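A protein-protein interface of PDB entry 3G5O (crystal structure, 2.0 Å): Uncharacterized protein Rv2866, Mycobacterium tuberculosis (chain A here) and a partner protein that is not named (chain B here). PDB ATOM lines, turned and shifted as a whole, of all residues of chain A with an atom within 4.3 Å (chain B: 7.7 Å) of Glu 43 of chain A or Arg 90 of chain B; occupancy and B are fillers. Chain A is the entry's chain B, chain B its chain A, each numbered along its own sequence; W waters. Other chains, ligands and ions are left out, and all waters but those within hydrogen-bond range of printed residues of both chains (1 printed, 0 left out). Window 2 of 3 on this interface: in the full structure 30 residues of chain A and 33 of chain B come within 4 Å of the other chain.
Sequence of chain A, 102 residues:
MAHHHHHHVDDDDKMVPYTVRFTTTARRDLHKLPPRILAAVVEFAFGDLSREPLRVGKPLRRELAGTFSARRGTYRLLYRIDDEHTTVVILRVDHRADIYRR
Of the 9 printed residues of chain A, 4 touch a printed residue of chain B.
The guanidinium group (NH1) of Arg 90 of chain B is in salt-bridge range of the side-chain carboxylate (OE2) of Glu 43 of chain A (2.9 Å).
Water W1 lies within hydrogen-bond range of the side-chain carboxylate of Glu 86 of chain B, the guanidinium group of Arg 90 of chain B and the backbone carbonyl oxygen of Phe 46 of chain A.
Of the printed residues of chain B, Val 42 of chain A touches Ile 89 and Arg 90. Printed residues of chain B within 4 Å of Glu 43 of chain A: Arg 90 and Val 95. Of chain A, only Val 42 and Glu 43 come within 4 Å of Arg 90 of chain B. Of the printed residues of chain A, Val 95 of chain B touches Ala 39 (3.98 Å) and Glu 43 (3.4 Å). The nearest residue of chain B that does not touch Glu 43 of chain A is Pro 96 of chain B (4.04 Å). The nearest printed residue of chain A that does not touch Arg 90 of chain B is Phe 46 of chain A (4.4 Å).
Among the printed residues, merely in contact across the chains: Ala 39 of chain A with Val 95 of chain B (3.98 Å), Val 42 of chain A with Ile 89 of chain B (3.9 Å), Val 42 of chain A with Arg 90 of chain B (3.8 Å), Glu 43 of chain A with Val 95 of chain B (3.4 Å), Phe 46 of chain A with Glu 86 of chain B (3.5 Å) and Phe 46 of chain A with Ile 89 of chain B (3.96 Å).
OE2 of Glu 86 of chain B is in salt-bridge range of NH1 of Arg 97 of chain B (3.1 Å). The guanidinium group (NE) of Arg 90 of chain B is in salt-bridge range of the side-chain carboxylate (OE2) of Glu 86 of chain B (2.8 Å). The backbone carbonyl oxygen (O) of Val 95 of chain B lies within hydrogen-bond range of the guanidinium group (NH1) of Arg 90 of chain B, 2.8 Å away.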
ATOM      1  N   ALA A  39       6.975  21.157   8.733  1.00  0.00           N
ATOM      2  CA  ALA A  39       6.533  20.400   9.905  1.00  0.00           C
ATOM      3  C   ALA A  39       5.391  19.409   9.569  1.00  0.00           C
ATOM      4  O   ALA A  39       5.350  18.326  10.106  1.00  0.00           O
ATOM      5  CB  ALA A  39       6.175  21.346  11.111  1.00  0.00           C
ATOM      6  N   ALA A  40       4.536  19.770   8.614  1.00  0.00           N
ATOM      7  CA  ALA A  40       3.368  18.972   8.268  1.00  0.00           C
ATOM      8  C   ALA A  40       3.844  17.713   7.555  1.00  0.00           C
ATOM      9  O   ALA A  40       3.389  16.614   7.838  1.00  0.00           O
ATOM     10  CB  ALA A  40       2.440  19.791   7.329  1.00  0.00           C
ATOM     11  N   VAL A  41       4.808  17.901   6.655  1.00  0.00           N
ATOM     12  CA  VAL A  41       5.451  16.814   5.942  1.00  0.00           C
ATOM     13  C   VAL A  41       6.096  15.853   6.939  1.00  0.00           C
ATOM     14  O   VAL A  41       5.916  14.649   6.832  1.00  0.00           O
ATOM     15  CB  VAL A  41       6.510  17.366   4.952  1.00  0.00           C
ATOM     16  CG1 VAL A  41       7.441  16.233   4.424  1.00  0.00           C
ATOM     17  CG2 VAL A  41       5.804  18.071   3.766  1.00  0.00           C
ATOM     18  N   VAL A  42       6.867  16.378   7.887  1.00  0.00           N
ATOM     19  CA  VAL A  42       7.526  15.507   8.888  1.00  0.00           C
ATOM     20  C   VAL A  42       6.497  14.701   9.716  1.00  0.00           C
ATOM     21  O   VAL A  42       6.650  13.477   9.908  1.00  0.00           O
ATOM     22  CB  VAL A  42       8.487  16.311   9.753  1.00  0.00           C
ATOM     23  CG1 VAL A  42       8.962  15.495  10.945  1.00  0.00           C
ATOM     24  CG2 VAL A  42       9.709  16.771   8.904  1.00  0.00           C
ATOM     25  N   GLU A  43       5.424  15.358  10.155  1.00  0.00           N
ATOM     26  CA  GLU A  43       4.404  14.644  10.935  1.00  0.00           C
ATOM     27  C   GLU A  43       3.688  13.581  10.118  1.00  0.00           C
ATOM     28  O   GLU A  43       3.414  12.505  10.594  1.00  0.00           O
ATOM     29  CB  GLU A  43       3.424  15.619  11.603  1.00  0.00           C
ATOM     30  CG  GLU A  43       4.115  16.608  12.561  1.00  0.00           C
ATOM     31  CD  GLU A  43       4.818  15.955  13.777  1.00  0.00           C
ATOM     32  OE1 GLU A  43       4.516  14.795  14.112  1.00  0.00           O
ATOM     33  OE2 GLU A  43       5.680  16.616  14.393  1.00  0.00           O
ATOM     34  N   PHE A  44       3.406  13.864   8.862  1.00  0.00           N
ATOM     35  CA  PHE A  44       2.781  12.851   8.021  1.00  0.00           C
ATOM     36  C   PHE A  44       3.745  11.683   7.740  1.00  0.00           C
ATOM     37  O   PHE A  44       3.360  10.521   7.859  1.00  0.00           O
ATOM     38  CB  PHE A  44       2.355  13.502   6.679  1.00  0.00           C
ATOM     39  CG  PHE A  44       1.856  12.528   5.671  1.00  0.00           C
ATOM     40  CD1 PHE A  44       0.642  11.860   5.865  1.00  0.00           C
ATOM     41  CD2 PHE A  44       2.588  12.293   4.490  1.00  0.00           C
ATOM     42  CE1 PHE A  44       0.185  10.894   4.947  1.00  0.00           C
ATOM     43  CE2 PHE A  44       2.136  11.370   3.551  1.00  0.00           C
ATOM     44  CZ  PHE A  44       0.918  10.666   3.770  1.00  0.00           C
ATOM     45  N   ALA A  45       4.960  12.014   7.297  1.00  0.00           N
ATOM     46  CA  ALA A  45       5.957  11.007   6.940  1.00  0.00           C
ATOM     47  C   ALA A  45       6.209  10.004   8.062  1.00  0.00           C
ATOM     48  O   ALA A  45       6.308   8.806   7.812  1.00  0.00           O
ATOM     49  CB  ALA A  45       7.300  11.709   6.537  1.00  0.00           C
ATOM     50  N   PHE A  46       6.297  10.481   9.307  1.00  0.00           N
ATOM     51  CA  PHE A  46       6.605   9.580  10.419  1.00  0.00           C
ATOM     52  C   PHE A  46       5.362   9.159  11.206  1.00  0.00           C
ATOM     53  O   PHE A  46       5.469   8.506  12.238  1.00  0.00           O
ATOM     54  CB  PHE A  46       7.713  10.156  11.319  1.00  0.00           C
ATOM     55  CG  PHE A  46       8.977  10.483  10.565  1.00  0.00           C
ATOM     56  CD1 PHE A  46       9.715   9.479   9.950  1.00  0.00           C
ATOM     57  CD2 PHE A  46       9.420  11.796  10.464  1.00  0.00           C
ATOM     58  CE1 PHE A  46      10.904   9.781   9.225  1.00  0.00           C
ATOM     59  CE2 PHE A  46      10.593  12.115   9.724  1.00  0.00           C
ATOM     60  CZ  PHE A  46      11.333  11.100   9.125  1.00  0.00           C
ATOM     61  N   GLY A  47       4.185   9.510  10.678  1.00  0.00           N
ATOM     62  CA  GLY A  47       2.892   9.158  11.281  1.00  0.00           C
ATOM     63  C   GLY A  47       2.120   8.276  10.336  1.00  0.00           C
ATOM     64  O   GLY A  47       2.413   7.070  10.211  1.00  0.00           O
ATOM     65  N   GLY B  85      16.673   8.943   8.916  1.00  0.00           N
ATOM     66  CA  GLY B  85      15.429   8.491   9.582  1.00  0.00           C
ATOM     67  C   GLY B  85      14.818   9.555  10.485  1.00  0.00           C
ATOM     68  O   GLY B  85      15.303  10.679  10.551  1.00  0.00           O
ATOM     69  N   GLU B  86      13.772   9.172  11.217  1.00  0.00           N
ATOM     70  CA  GLU B  86      12.987  10.110  12.010  1.00  0.00           C
ATOM     71  C   GLU B  86      13.784  10.975  12.979  1.00  0.00           C
ATOM     72  O   GLU B  86      13.617  12.211  12.983  1.00  0.00           O
ATOM     73  CB  GLU B  86      11.902   9.364  12.782  1.00  0.00           C
ATOM     74  CG  GLU B  86      11.101  10.329  13.666  1.00  0.00           C
ATOM     75  CD  GLU B  86       9.850   9.695  14.257  1.00  0.00           C
ATOM     76  OE1 GLU B  86       9.681   8.456  14.153  1.00  0.00           O
ATOM     77  OE2 GLU B  86       9.024  10.454  14.816  1.00  0.00           O
ATOM     78  N   ASP B  87      14.638  10.360  13.797  1.00  0.00           N
ATOM     79  CA  ASP B  87      15.349  11.166  14.811  1.00  0.00           C
ATOM     80  C   ASP B  87      16.257  12.191  14.165  1.00  0.00           C
ATOM     81  O   ASP B  87      16.262  13.348  14.586  1.00  0.00           O
ATOM     82  CB  ASP B  87      16.115  10.305  15.868  1.00  0.00           C
ATOM     83  CG  ASP B  87      15.168   9.439  16.714  1.00  0.00           C
ATOM     84  OD1 ASP B  87      14.017   9.875  16.972  1.00  0.00           O
ATOM     85  OD2 ASP B  87      15.557   8.290  17.090  1.00  0.00           O
ATOM     86  N   GLU B  88      16.979  11.794  13.112  1.00  0.00           N
ATOM     87  CA  GLU B  88      17.844  12.719  12.432  1.00  0.00           C
ATOM     88  C   GLU B  88      17.093  13.873  11.774  1.00  0.00           C
ATOM     89  O   GLU B  88      17.528  15.030  11.850  1.00  0.00           O
ATOM     90  CB  GLU B  88      18.677  12.009  11.358  1.00  0.00           C
ATOM     91  CG  GLU B  88      19.604  10.928  11.897  1.00  0.00           C
ATOM     92  CD  GLU B  88      19.875   9.870  10.835  1.00  0.00           C
ATOM     93  OE1 GLU B  88      18.996   9.026  10.538  1.00  0.00           O
ATOM     94  OE2 GLU B  88      20.979   9.912  10.262  1.00  0.00           O
ATOM     95  N   ILE B  89      15.983  13.556  11.108  1.00  0.00           N
ATOM     96  CA  ILE B  89      15.229  14.574  10.403  1.00  0.00           C
ATOM     97  C   ILE B  89      14.583  15.529  11.417  1.00  0.00           C
ATOM     98  O   ILE B  89      14.630  16.735  11.227  1.00  0.00           O
ATOM     99  CB  ILE B  89      14.145  13.944   9.456  1.00  0.00           C
ATOM    100  CG1 ILE B  89      14.784  13.220   8.272  1.00  0.00           C
ATOM    101  CG2 ILE B  89      13.164  15.019   8.922  1.00  0.00           C
ATOM    102  CD1 ILE B  89      15.409  14.118   7.226  1.00  0.00           C
ATOM    103  N   ARG B  90      13.968  14.989  12.480  1.00  0.00           N
ATOM    104  CA  ARG B  90      13.331  15.828  13.505  1.00  0.00           C
ATOM    105  C   ARG B  90      14.347  16.753  14.160  1.00  0.00           C
ATOM    106  O   ARG B  90      14.076  17.948  14.364  1.00  0.00           O
ATOM    107  CB  ARG B  90      12.609  14.982  14.559  1.00  0.00           C
ATOM    108  CG  ARG B  90      11.322  14.278  14.043  1.00  0.00           C
ATOM    109  CD  ARG B  90      10.542  13.804  15.212  1.00  0.00           C
ATOM    110  NE  ARG B  90       9.253  13.196  14.864  1.00  0.00           N
ATOM    111  CZ  ARG B  90       8.149  13.901  14.612  1.00  0.00           C
ATOM    112  NH1 ARG B  90       8.192  15.240  14.649  1.00  0.00           N
ATOM    113  NH2 ARG B  90       6.996  13.267  14.349  1.00  0.00           N
ATOM    114  N   ALA B  91      15.532  16.229  14.447  1.00  0.00           N
ATOM    115  CA  ALA B  91      16.565  17.089  15.025  1.00  0.00           C
ATOM    116  C   ALA B  91      17.154  18.091  14.039  1.00  0.00           C
ATOM    117  O   ALA B  91      17.365  19.234  14.402  1.00  0.00           O
ATOM    118  CB  ALA B  91      17.680  16.254  15.717  1.00  0.00           C
ATOM    119  N   GLU B  92      17.389  17.725  12.784  1.00  0.00           N
ATOM    120  CA  GLU B  92      17.935  18.742  11.866  1.00  0.00           C
ATOM    121  C   GLU B  92      16.942  19.886  11.569  1.00  0.00           C
ATOM    122  O   GLU B  92      17.341  21.044  11.382  1.00  0.00           O
ATOM    123  CB  GLU B  92      18.374  18.109  10.543  1.00  0.00           C
ATOM    124  CG  GLU B  92      18.840  19.094   9.478  1.00  0.00           C
ATOM    125  CD  GLU B  92      19.228  18.396   8.191  1.00  0.00           C
ATOM    126  OE1 GLU B  92      19.080  17.155   8.137  1.00  0.00           O
ATOM    127  OE2 GLU B  92      19.679  19.059   7.230  1.00  0.00           O
ATOM    128  N   PHE B  93      15.654  19.557  11.480  1.00  0.00           N
ATOM    129  CA  PHE B  93      14.691  20.563  11.049  1.00  0.00           C
ATOM    130  C   PHE B  93      13.916  21.199  12.194  1.00  0.00           C
ATOM    131  O   PHE B  93      13.089  22.068  11.945  1.00  0.00           O
ATOM    132  CB  PHE B  93      13.745  19.998   9.969  1.00  0.00           C
ATOM    133  CG  PHE B  93      14.414  19.790   8.645  1.00  0.00           C
ATOM    134  CD1 PHE B  93      14.647  20.871   7.795  1.00  0.00           C
ATOM    135  CD2 PHE B  93      14.836  18.535   8.253  1.00  0.00           C
ATOM    136  CE1 PHE B  93      15.276  20.682   6.570  1.00  0.00           C
ATOM    137  CE2 PHE B  93      15.473  18.346   7.034  1.00  0.00           C
ATOM    138  CZ  PHE B  93      15.693  19.421   6.187  1.00  0.00           C
ATOM    139  N   GLY B  94      14.191  20.767  13.426  1.00  0.00           N
ATOM    140  CA  GLY B  94      13.600  21.345  14.648  1.00  0.00           C
ATOM    141  C   GLY B  94      12.102  21.045  14.774  1.00  0.00           C
ATOM    142  O   GLY B  94      11.299  21.968  14.991  1.00  0.00           O
ATOM    143  N   VAL B  95      11.725  19.776  14.586  1.00  0.00           N
ATOM    144  CA  VAL B  95      10.316  19.351  14.682  1.00  0.00           C
ATOM    145  C   VAL B  95      10.290  18.180  15.637  1.00  0.00           C
ATOM    146  O   VAL B  95      10.241  17.036  15.183  1.00  0.00           O
ATOM    147  CB  VAL B  95       9.682  18.939  13.280  1.00  0.00           C
ATOM    148  CG1 VAL B  95       8.156  18.743  13.385  1.00  0.00           C
ATOM    149  CG2 VAL B  95      10.001  19.950  12.203  1.00  0.00           C
ATOM    150  N   PRO B  96      10.336  18.463  16.967  1.00  0.00           N
ATOM    151  CA  PRO B  96      10.359  17.420  17.980  1.00  0.00           C
ATOM    152  C   PRO B  96       9.031  16.666  18.062  1.00  0.00           C
ATOM    153  O   PRO B  96       7.987  17.182  17.666  1.00  0.00           O
ATOM    154  CB  PRO B  96      10.625  18.195  19.289  1.00  0.00           C
ATOM    155  CG  PRO B  96       9.962  19.515  19.072  1.00  0.00           C
ATOM    156  CD  PRO B  96      10.199  19.807  17.580  1.00  0.00           C
ATOM    157  N   ARG B  97       9.099  15.435  18.546  1.00  0.00           N
ATOM    158  CA  ARG B  97       7.922  14.618  18.778  1.00  0.00           C
ATOM    159  C   ARG B  97       7.177  15.124  20.023  1.00  0.00           C
ATOM    160  O   ARG B  97       7.647  16.030  20.713  1.00  0.00           O
ATOM    161  CB  ARG B  97       8.399  13.203  19.028  1.00  0.00           C
ATOM    162  CG  ARG B  97       7.567  12.086  18.432  1.00  0.00           C
ATOM    163  CD  ARG B  97       8.178  10.756  18.879  1.00  0.00           C
ATOM    164  NE  ARG B  97       9.623  10.831  18.686  1.00  0.00           N
ATOM    165  CZ  ARG B  97      10.341   9.992  17.948  1.00  0.00           C
ATOM    166  NH1 ARG B  97       9.770   8.943  17.362  1.00  0.00           N
ATOM    167  NH2 ARG B  97      11.642  10.196  17.822  1.00  0.00           N
ATOM    168  N   ARG B  98       6.007  14.539  20.283  1.00  0.00           N
ATOM    169  CA  ARG B  98       5.325  14.557  21.620  1.00  0.00           C
ATOM    170  C   ARG B  98       4.111  15.462  21.699  1.00  0.00           C
ATOM    171  O   ARG B  98       2.994  14.988  21.450  1.00  0.00           O
ATOM    172  CB  ARG B  98       6.283  14.794  22.819  1.00  0.00           C
ATOM    173  CG  ARG B  98       6.521  13.548  23.659  1.00  0.00           C
ATOM    174  CD  ARG B  98       7.676  12.721  23.119  1.00  0.00           C
ATOM    175  NE  ARG B  98       7.329  11.314  22.875  1.00  0.00           N
ATOM    176  CZ  ARG B  98       8.211  10.365  22.534  1.00  0.00           C
ATOM    177  NH1 ARG B  98       9.504  10.660  22.418  1.00  0.00           N
ATOM    178  NH2 ARG B  98       7.807   9.112  22.320  1.00  0.00           N
HETATM  179  O   HOH W   1       6.456  10.149  14.933  1.00  0.00           O
